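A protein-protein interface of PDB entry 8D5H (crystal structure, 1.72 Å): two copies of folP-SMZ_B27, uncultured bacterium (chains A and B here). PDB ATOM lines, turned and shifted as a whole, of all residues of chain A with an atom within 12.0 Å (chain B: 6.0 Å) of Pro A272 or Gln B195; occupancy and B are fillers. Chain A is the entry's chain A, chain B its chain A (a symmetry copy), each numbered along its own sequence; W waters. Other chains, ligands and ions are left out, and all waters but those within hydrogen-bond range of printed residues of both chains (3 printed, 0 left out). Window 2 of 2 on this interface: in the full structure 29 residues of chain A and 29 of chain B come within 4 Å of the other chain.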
ATOM      1  N   GLY A   2      22.659 -26.269 -23.236  1.00  0.00           N
ATOM      2  CA  GLY A   2      22.103 -26.989 -22.100  1.00  0.00           C
ATOM      3  C   GLY A   2      23.034 -26.943 -20.896  1.00  0.00           C
ATOM      4  O   GLY A   2      24.141 -27.473 -20.949  1.00  0.00           O
ATOM      5  N   MET A   3      22.601 -26.327 -19.852  1.00  0.00           N
ATOM      6  CA  MET A   3      23.430 -26.219 -18.716  1.00  0.00           C
ATOM      7  C   MET A   3      23.342 -27.499 -17.859  1.00  0.00           C
ATOM      8  O   MET A   3      22.276 -27.957 -17.596  1.00  0.00           O
ATOM      9  CB  MET A   3      23.049 -24.995 -17.884  1.00  0.00           C
ATOM     10  CG  MET A   3      23.941 -24.761 -16.675  1.00  0.00           C
ATOM     11  SD  MET A   3      25.633 -24.339 -17.130  1.00  0.00           S
ATOM     12  CE  MET A   3      25.425 -22.643 -17.669  1.00  0.00           C
ATOM     13  N   LEU A 244      22.650 -21.460  -8.350  1.00  0.00           N
ATOM     14  CA  LEU A 244      22.420 -20.284  -9.177  1.00  0.00           C
ATOM     15  C   LEU A 244      23.709 -19.472  -9.384  1.00  0.00           C
ATOM     16  O   LEU A 244      23.939 -18.890 -10.470  1.00  0.00           O
ATOM     17  CB  LEU A 244      21.340 -19.401  -8.532  1.00  0.00           C
ATOM     18  CG  LEU A 244      20.778 -18.311  -9.458  1.00  0.00           C
ATOM     19  CD1 LEU A 244      19.798 -18.894 -10.432  1.00  0.00           C
ATOM     20  CD2 LEU A 244      20.061 -17.281  -8.574  1.00  0.00           C
ATOM     21  N   GLU A 263      17.653 -28.462  -8.953  1.00  0.00           N
ATOM     22  CA  GLU A 263      17.222 -28.590 -10.336  1.00  0.00           C
ATOM     23  C   GLU A 263      16.509 -27.333 -10.777  1.00  0.00           C
ATOM     24  O   GLU A 263      16.637 -26.918 -11.944  1.00  0.00           O
ATOM     25  CB  GLU A 263      16.314 -29.815 -10.560  1.00  0.00           C
ATOM     26  CG  GLU A 263      15.555 -29.723 -11.865  1.00  0.00           C
ATOM     27  CD  GLU A 263      14.558 -30.886 -12.072  1.00  0.00           C
ATOM     28  OE1 GLU A 263      14.159 -31.504 -11.060  1.00  0.00           O
ATOM     29  OE2 GLU A 263      14.264 -31.250 -13.236  1.00  0.00           O
ATOM     30  N   ILE A 264      15.773 -26.706  -9.846  1.00  0.00           N
ATOM     31  CA  ILE A 264      15.049 -25.468 -10.156  1.00  0.00           C
ATOM     32  C   ILE A 264      16.030 -24.319 -10.389  1.00  0.00           C
ATOM     33  O   ILE A 264      15.873 -23.537 -11.336  1.00  0.00           O
ATOM     34  CB  ILE A 264      14.026 -25.138  -9.023  1.00  0.00           C
ATOM     35  CG1 ILE A 264      12.936 -26.225  -8.948  1.00  0.00           C
ATOM     36  CG2 ILE A 264      13.363 -23.725  -9.254  1.00  0.00           C
ATOM     37  CD1 ILE A 264      12.317 -26.659 -10.303  1.00  0.00           C
ATOM     38  N   ALA A 265      17.089 -24.238  -9.587  1.00  0.00           N
ATOM     39  CA  ALA A 265      18.144 -23.267  -9.817  1.00  0.00           C
ATOM     40  C   ALA A 265      18.779 -23.457 -11.199  1.00  0.00           C
ATOM     41  O   ALA A 265      19.001 -22.487 -11.936  1.00  0.00           O
ATOM     42  CB  ALA A 265      19.203 -23.405  -8.692  1.00  0.00           C
ATOM     43  N   THR A 266      19.084 -24.710 -11.561  1.00  0.00           N
ATOM     44  CA  THR A 266      19.655 -24.971 -12.884  1.00  0.00           C
ATOM     45  C   THR A 266      18.718 -24.479 -13.984  1.00  0.00           C
ATOM     46  O   THR A 266      19.153 -23.881 -14.992  1.00  0.00           O
ATOM     47  CB  THR A 266      19.951 -26.476 -13.013  1.00  0.00           C
ATOM     48  OG1 THR A 266      20.854 -26.872 -11.997  1.00  0.00           O
ATOM     49  CG2 THR A 266      20.529 -26.782 -14.404  1.00  0.00           C
ATOM     50  N   ALA A 267      17.409 -24.717 -13.823  1.00  0.00           N
ATOM     51  CA  ALA A 267      16.465 -24.306 -14.850  1.00  0.00           C
ATOM     52  C   ALA A 267      16.417 -22.778 -14.978  1.00  0.00           C
ATOM     53  O   ALA A 267      16.247 -22.239 -16.076  1.00  0.00           O
ATOM     54  CB  ALA A 267      15.067 -24.866 -14.538  1.00  0.00           C
ATOM     55  N   ILE A 268      16.502 -22.085 -13.865  1.00  0.00           N
ATOM     56  CA  ILE A 268      16.552 -20.621 -13.902  1.00  0.00           C
ATOM     57  C   ILE A 268      17.832 -20.140 -14.619  1.00  0.00           C
ATOM     58  O   ILE A 268      17.801 -19.143 -15.347  1.00  0.00           O
ATOM     59  CB  ILE A 268      16.434 -20.106 -12.450  1.00  0.00           C
ATOM     60  CG1 ILE A 268      14.996 -20.383 -11.959  1.00  0.00           C
ATOM     61  CG2 ILE A 268      16.729 -18.532 -12.395  1.00  0.00           C
ATOM     62  CD1 ILE A 268      14.753 -20.238 -10.389  1.00  0.00           C
ATOM     63  N   ASN A 269      18.954 -20.840 -14.435  1.00  0.00           N
ATOM     64  CA  ASN A 269      20.204 -20.509 -15.140  1.00  0.00           C
ATOM     65  C   ASN A 269      20.178 -20.864 -16.610  1.00  0.00           C
ATOM     66  O   ASN A 269      21.090 -20.462 -17.353  1.00  0.00           O
ATOM     67  CB  ASN A 269      21.346 -21.242 -14.481  1.00  0.00           C
ATOM     68  CG  ASN A 269      21.959 -20.417 -13.394  1.00  0.00           C
ATOM     69  OD1 ASN A 269      21.739 -19.198 -13.346  1.00  0.00           O
ATOM     70  ND2 ASN A 269      22.786 -21.033 -12.591  1.00  0.00           N
ATOM     71  N   GLN A 270      19.158 -21.575 -17.076  1.00  0.00           N
ATOM     72  CA  GLN A 270      19.166 -22.056 -18.439  1.00  0.00           C
ATOM     73  C   GLN A 270      18.722 -20.947 -19.400  1.00  0.00           C
ATOM     74  O   GLN A 270      17.574 -20.478 -19.310  1.00  0.00           O
ATOM     75  CB  GLN A 270      18.270 -23.299 -18.508  1.00  0.00           C
ATOM     76  CG  GLN A 270      18.056 -23.859 -19.901  1.00  0.00           C
ATOM     77  CD  GLN A 270      19.364 -24.270 -20.554  1.00  0.00           C
ATOM     78  OE1 GLN A 270      20.025 -25.199 -20.090  1.00  0.00           O
ATOM     79  NE2 GLN A 270      19.753 -23.563 -21.623  1.00  0.00           N
ATOM     80  N   PRO A 271      19.589 -20.472 -20.293  1.00  0.00           N
ATOM     81  CA  PRO A 271      19.192 -19.422 -21.249  1.00  0.00           C
ATOM     82  C   PRO A 271      18.140 -19.926 -22.219  1.00  0.00           C
ATOM     83  O   PRO A 271      18.017 -21.142 -22.444  1.00  0.00           O
ATOM     84  CB  PRO A 271      20.505 -19.085 -21.974  1.00  0.00           C
ATOM     85  CG  PRO A 271      21.357 -20.256 -21.775  1.00  0.00           C
ATOM     86  CD  PRO A 271      21.022 -20.802 -20.421  1.00  0.00           C
ATOM     87  N   PRO A 272      17.371 -19.016 -22.803  1.00  0.00           N
ATOM     88  CA  PRO A 272      16.326 -19.395 -23.757  1.00  0.00           C
ATOM     89  C   PRO A 272      16.908 -20.047 -25.000  1.00  0.00           C
ATOM     90  O   PRO A 272      18.123 -20.087 -25.233  1.00  0.00           O
ATOM     91  CB  PRO A 272      15.646 -18.071 -24.131  1.00  0.00           C
ATOM     92  CG  PRO A 272      16.330 -17.010 -23.413  1.00  0.00           C
ATOM     93  CD  PRO A 272      17.496 -17.556 -22.635  1.00  0.00           C
ATOM     94  N   GLU A 273      15.985 -20.565 -25.803  1.00  0.00           N
ATOM     95  CA  GLU A 273      16.322 -21.225 -27.051  1.00  0.00           C
ATOM     96  C   GLU A 273      17.058 -20.255 -27.965  1.00  0.00           C
ATOM     97  O   GLU A 273      16.642 -19.104 -28.137  1.00  0.00           O
ATOM     98  CB  GLU A 273      15.046 -21.744 -27.711  1.00  0.00           C
ATOM     99  CG  GLU A 273      14.464 -22.979 -27.018  1.00  0.00           C
ATOM    100  CD  GLU A 273      12.947 -23.121 -27.195  1.00  0.00           C
ATOM    101  OE1 GLU A 273      12.349 -22.391 -28.020  1.00  0.00           O
ATOM    102  OE2 GLU A 273      12.345 -23.957 -26.493  1.00  0.00           O
ATOM    103  N   ARG A 274      18.168 -20.723 -28.528  1.00  0.00           N
ATOM    104  CA  ARG A 274      19.071 -19.886 -29.307  1.00  0.00           C
ATOM    105  C   ARG A 274      18.807 -20.027 -30.802  1.00  0.00           C
ATOM    106  O   ARG A 274      18.455 -21.104 -31.294  1.00  0.00           O
ATOM    107  CB  ARG A 274      20.524 -20.248 -28.986  1.00  0.00           C
ATOM    108  CG  ARG A 274      21.407 -19.070 -28.574  1.00  0.00           C
ATOM    109  CD  ARG A 274      22.818 -19.544 -28.220  1.00  0.00           C
ATOM    110  NE  ARG A 274      23.415 -20.342 -29.288  1.00  0.00           N
ATOM    111  CZ  ARG A 274      23.910 -21.564 -29.129  1.00  0.00           C
ATOM    112  NH1 ARG A 274      23.916 -22.160 -27.947  1.00  0.00           N
ATOM    113  NH2 ARG A 274      24.411 -22.203 -30.184  1.00  0.00           N
ATOM    114  OXT ARG A 274      18.947 -19.061 -31.550  1.00  0.00           O
ATOM    115  N   VAL B 149       9.337 -15.040 -28.242  1.00  0.00           N
ATOM    116  CA  VAL B 149      10.674 -14.656 -28.712  1.00  0.00           C
ATOM    117  C   VAL B 149      11.506 -14.169 -27.543  1.00  0.00           C
ATOM    118  O   VAL B 149      12.719 -14.435 -27.463  1.00  0.00           O
ATOM    119  CB  VAL B 149      10.569 -13.563 -29.785  1.00  0.00           C
ATOM    120  CG1 VAL B 149      11.961 -12.988 -30.141  1.00  0.00           C
ATOM    121  CG2 VAL B 149       9.914 -14.154 -31.053  1.00  0.00           C
ATOM    122  N   ASP B 150      10.873 -13.432 -26.627  1.00  0.00           N
ATOM    123  CA  ASP B 150      11.573 -12.828 -25.476  1.00  0.00           C
ATOM    124  C   ASP B 150      10.512 -12.548 -24.400  1.00  0.00           C
ATOM    125  O   ASP B 150       9.878 -11.483 -24.399  1.00  0.00           O
ATOM    126  CB  ASP B 150      12.299 -11.548 -25.908  1.00  0.00           C
ATOM    127  CG  ASP B 150      13.094 -10.901 -24.768  1.00  0.00           C
ATOM    128  OD1 ASP B 150      12.943 -11.277 -23.585  1.00  0.00           O
ATOM    129  OD2 ASP B 150      13.872 -10.005 -25.077  1.00  0.00           O
ATOM    130  N   VAL B 151      10.242 -13.557 -23.570  1.00  0.00           N
ATOM    131  CA  VAL B 151       9.099 -13.420 -22.643  1.00  0.00           C
ATOM    132  C   VAL B 151       9.335 -12.261 -21.684  1.00  0.00           C
ATOM    133  O   VAL B 151       8.377 -11.602 -21.243  1.00  0.00           O
ATOM    134  CB  VAL B 151       8.819 -14.745 -21.895  1.00  0.00           C
ATOM    135  CG1 VAL B 151       9.953 -15.063 -20.910  1.00  0.00           C
ATOM    136  CG2 VAL B 151       7.444 -14.707 -21.140  1.00  0.00           C
ATOM    137  N   VAL B 152      10.591 -11.970 -21.349  1.00  0.00           N
ATOM    138  CA  VAL B 152      10.855 -10.857 -20.421  1.00  0.00           C
ATOM    139  C   VAL B 152      10.417  -9.531 -21.044  1.00  0.00           C
ATOM    140  O   VAL B 152       9.779  -8.698 -20.379  1.00  0.00           O
ATOM    141  CB  VAL B 152      12.341 -10.834 -20.025  1.00  0.00           C
ATOM    142  CG1 VAL B 152      12.651  -9.596 -19.184  1.00  0.00           C
ATOM    143  CG2 VAL B 152      12.663 -12.103 -19.213  1.00  0.00           C
ATOM    144  N   PRO B 190       7.064 -24.681 -19.294  1.00  0.00           N
ATOM    145  CA  PRO B 190       7.663 -24.128 -18.068  1.00  0.00           C
ATOM    146  C   PRO B 190       8.853 -23.216 -18.304  1.00  0.00           C
ATOM    147  O   PRO B 190       9.178 -22.451 -17.403  1.00  0.00           O
ATOM    148  CB  PRO B 190       8.082 -25.392 -17.273  1.00  0.00           C
ATOM    149  CG  PRO B 190       8.155 -26.461 -18.260  1.00  0.00           C
ATOM    150  CD  PRO B 190       7.168 -26.152 -19.353  1.00  0.00           C
ATOM    151  N   GLN B 191       9.534 -23.278 -19.465  1.00  0.00           N
ATOM    152  CA  GLN B 191      10.800 -22.550 -19.576  1.00  0.00           C
ATOM    153  C   GLN B 191      10.602 -21.057 -19.344  1.00  0.00           C
ATOM    154  O   GLN B 191      11.456 -20.407 -18.734  1.00  0.00           O
ATOM    155  CB  GLN B 191      11.439 -22.808 -20.925  1.00  0.00           C
ATOM    156  CG  GLN B 191      10.658 -22.187 -22.079  1.00  0.00           C
ATOM    157  CD  GLN B 191      11.395 -22.373 -23.391  1.00  0.00           C
ATOM    158  OE1 GLN B 191      12.530 -21.900 -23.554  1.00  0.00           O
ATOM    159  NE2 GLN B 191      10.783 -23.073 -24.325  1.00  0.00           N
ATOM    160  N   TYR B 192       9.417 -20.540 -19.691  1.00  0.00           N
ATOM    161  CA  TYR B 192       9.221 -19.102 -19.609  1.00  0.00           C
ATOM    162  C   TYR B 192       9.079 -18.625 -18.173  1.00  0.00           C
ATOM    163  O   TYR B 192       9.471 -17.479 -17.864  1.00  0.00           O
ATOM    164  CB  TYR B 192       8.019 -18.724 -20.481  1.00  0.00           C
ATOM    165  CG  TYR B 192       8.327 -19.077 -21.937  1.00  0.00           C
ATOM    166  CD1 TYR B 192       9.363 -18.411 -22.642  1.00  0.00           C
ATOM    167  CD2 TYR B 192       7.641 -20.117 -22.589  1.00  0.00           C
ATOM    168  CE1 TYR B 192       9.672 -18.743 -23.962  1.00  0.00           C
ATOM    169  CE2 TYR B 192       7.936 -20.468 -23.922  1.00  0.00           C
ATOM    170  CZ  TYR B 192       8.973 -19.785 -24.593  1.00  0.00           C
ATOM    171  OH  TYR B 192       9.254 -20.065 -25.885  1.00  0.00           O
ATOM    172  N   SER B 193       8.535 -19.476 -17.278  1.00  0.00           N
ATOM    173  CA  SER B 193       8.482 -19.120 -15.859  1.00  0.00           C
ATOM    174  C   SER B 193       9.884 -19.026 -15.271  1.00  0.00           C
ATOM    175  O   SER B 193      10.197 -18.092 -14.497  1.00  0.00           O
ATOM    176  CB  SER B 193       7.620 -20.149 -15.105  1.00  0.00           C
ATOM    177  OG  SER B 193       6.249 -20.031 -15.514  1.00  0.00           O
ATOM    178  N   PHE B 194      10.758 -19.961 -15.654  1.00  0.00           N
ATOM    179  CA  PHE B 194      12.116 -19.909 -15.135  1.00  0.00           C
ATOM    180  C   PHE B 194      12.852 -18.670 -15.638  1.00  0.00           C
ATOM    181  O   PHE B 194      13.673 -18.097 -14.904  1.00  0.00           O
ATOM    182  CB  PHE B 194      12.854 -21.173 -15.546  1.00  0.00           C
ATOM    183  CG  PHE B 194      12.308 -22.423 -14.910  1.00  0.00           C
ATOM    184  CD1 PHE B 194      12.248 -22.528 -13.513  1.00  0.00           C
ATOM    185  CD2 PHE B 194      11.882 -23.492 -15.704  1.00  0.00           C
ATOM    186  CE1 PHE B 194      11.752 -23.701 -12.861  1.00  0.00           C
ATOM    187  CE2 PHE B 194      11.414 -24.662 -15.081  1.00  0.00           C
ATOM    188  CZ  PHE B 194      11.325 -24.771 -13.688  1.00  0.00           C
ATOM    189  N   GLN B 195      12.594 -18.279 -16.895  1.00  0.00           N
ATOM    190  CA  GLN B 195      13.236 -17.105 -17.480  1.00  0.00           C
ATOM    191  C   GLN B 195      12.803 -15.837 -16.752  1.00  0.00           C
ATOM    192  O   GLN B 195      13.626 -14.932 -16.513  1.00  0.00           O
ATOM    193  CB  GLN B 195      12.941 -17.037 -18.977  1.00  0.00           C
ATOM    194  CG  GLN B 195      13.713 -18.116 -19.746  1.00  0.00           C
ATOM    195  CD  GLN B 195      13.145 -18.311 -21.127  1.00  0.00           C
ATOM    196  OE1 GLN B 195      12.502 -17.402 -21.669  1.00  0.00           O
ATOM    197  NE2 GLN B 195      13.399 -19.476 -21.727  1.00  0.00           N
ATOM    198  N   LEU B 196      11.516 -15.743 -16.409  1.00  0.00           N
ATOM    199  CA  LEU B 196      11.040 -14.583 -15.648  1.00  0.00           C
ATOM    200  C   LEU B 196      11.675 -14.530 -14.257  1.00  0.00           C
ATOM    201  O   LEU B 196      12.050 -13.455 -13.783  1.00  0.00           O
ATOM    202  CB  LEU B 196       9.510 -14.631 -15.517  1.00  0.00           C
ATOM    203  CG  LEU B 196       8.781 -14.305 -16.847  1.00  0.00           C
ATOM    204  CD1 LEU B 196       7.288 -14.702 -16.751  1.00  0.00           C
ATOM    205  CD2 LEU B 196       8.924 -12.793 -17.238  1.00  0.00           C
ATOM    206  N   LEU B 197      11.832 -15.688 -13.588  1.00  0.00           N
ATOM    207  CA  LEU B 197      12.508 -15.693 -12.297  1.00  0.00           C
ATOM    208  C   LEU B 197      13.971 -15.257 -12.446  1.00  0.00           C
ATOM    209  O   LEU B 197      14.511 -14.558 -11.571  1.00  0.00           O
ATOM    210  CB  LEU B 197      12.441 -17.092 -11.663  1.00  0.00           C
ATOM    211  CG  LEU B 197      11.028 -17.414 -11.230  1.00  0.00           C
ATOM    212  CD1 LEU B 197      11.015 -18.948 -10.947  1.00  0.00           C
ATOM    213  CD2 LEU B 197      10.701 -16.610  -9.907  1.00  0.00           C
ATOM    214  N   ALA B 198      14.614 -15.685 -13.533  1.00  0.00           N
ATOM    215  CA  ALA B 198      16.029 -15.367 -13.770  1.00  0.00           C
ATOM    216  C   ALA B 198      16.227 -13.871 -13.922  1.00  0.00           C
ATOM    217  O   ALA B 198      17.262 -13.313 -13.487  1.00  0.00           O
ATOM    218  CB  ALA B 198      16.536 -16.074 -15.038  1.00  0.00           C
ATOM    219  N   HIS B 199      15.254 -13.208 -14.543  1.00  0.00           N
ATOM    220  CA  HIS B 199      15.358 -11.802 -14.931  1.00  0.00           C
ATOM    221  C   HIS B 199      14.420 -10.920 -14.139  1.00  0.00           C
ATOM    222  O   HIS B 199      14.136  -9.782 -14.559  1.00  0.00           O
ATOM    223  CB  HIS B 199      15.079 -11.681 -16.428  1.00  0.00           C
ATOM    224  CG  HIS B 199      16.154 -12.281 -17.253  1.00  0.00           C
ATOM    225  ND1 HIS B 199      17.344 -11.630 -17.476  1.00  0.00           N
ATOM    226  CD2 HIS B 199      16.267 -13.495 -17.838  1.00  0.00           C
ATOM    227  CE1 HIS B 199      18.142 -12.408 -18.181  1.00  0.00           C
ATOM    228  NE2 HIS B 199      17.522 -13.550 -18.401  1.00  0.00           N
ATOM    229  N   LEU B 200      13.953 -11.388 -12.978  1.00  0.00           N
ATOM    230  CA  LEU B 200      12.988 -10.595 -12.218  1.00  0.00           C
ATOM    231  C   LEU B 200      13.539  -9.205 -11.870  1.00  0.00           C
ATOM    232  O   LEU B 200      12.771  -8.225 -11.837  1.00  0.00           O
ATOM    233  CB  LEU B 200      12.569 -11.369 -10.949  1.00  0.00           C
ATOM    234  CG  LEU B 200      11.478 -10.694 -10.135  1.00  0.00           C
ATOM    235  CD1 LEU B 200      10.199 -10.568 -10.967  1.00  0.00           C
ATOM    236  CD2 LEU B 200      11.247 -11.508  -8.851  1.00  0.00           C
HETATM  237  O   HOH W   1      15.154 -21.412 -20.446  1.00  0.00           O
HETATM  238  O   HOH W   2      14.690 -17.263 -27.624  1.00  0.00           O
HETATM  239  O   HOH W   3      12.920 -19.995 -25.232  1.00  0.00           O
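NE2 of Gln B191 lies within hydrogen-bond range of OE2 of Glu A273 (2.8 Å).
The side-chain amide oxygen (OE1) of Gln B191 is in hydrogen-bond range of the side-chain amide nitrogen (NE2) of Gln B195.
Among the printed residues, merely in contact across the chains: Ile A264 with Phe B194, Ala A267 with Phe B194, Ile A268 with Phe B194, Ile A268 with Leu B197, Ile A268 with Ala B198 and Pro A272 with Gln B195.
Of chain A, only Pro A272 (3.6 Å) comes within 4 Å of Gln B195. No residue of chain A comes within 4 Å of Val B151. No residue of chain A comes within 4 Å of Tyr B192. No residue of chain A comes within 4 Å of Ser B193. Phe B194 touches just these residues of chain A: Ile A264, Ala A267 and Ile A268. No residue of chain A comes within 4 Å of Leu B196. No residue of chain A comes within 4 Å of His B199. Printed residues of chain B within 4 Å of Ala A267: Phe B194. Printed residues of chain B within 4 Å of Ile A264: Phe B194. Of the printed residues of chain B, Glu A273 touches Gln B191 (2.8 Å). Of the printed residues of chain B, Ile A268 touches Phe B194, Leu B197 and Ala B198. Of the printed residues of chain A, Leu B197 touches Ile A268. The nearest residue of chain A that does not touch Gln B195 is Gln A270 (4.5 Å).
Of the 15 printed residues of chain A, 5 touch a printed residue of chain B. Hydrophobic or aromatic side chains of chain A within 4 Å of the printed part of chain B: Ile A264, Ala A267, Ile A268 and Pro A272. Of the 15 printed residues of chain B, 5 touch a printed residue of chain A. Hydrophobic or aromatic side chains of chain B that line the printed part of chain A: Phe B194, Leu B197 and Ala B198. Among the printed residues, 7 pairs touch across the chains. Among the printed residues, no Asp or Glu carboxylate lies within 4 Å of a Lys or Arg side-chain nitrogen of the other chain.
No position is printed for both chains.
Water W3 lies within hydrogen-bond range of OE1 of Gln B191 (2.6 Å) and N of Glu A273 (3.2 Å). Water W2 lies within hydrogen-bond range of O of Glu A273 and O of Val B149. Water W1 lies within hydrogen-bond range of the backbone carbonyl oxygen (O) of Gln A270 (2.8 Å) and the side-chain amide nitrogen (NE2) of Gln B195 (2.9 Å).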
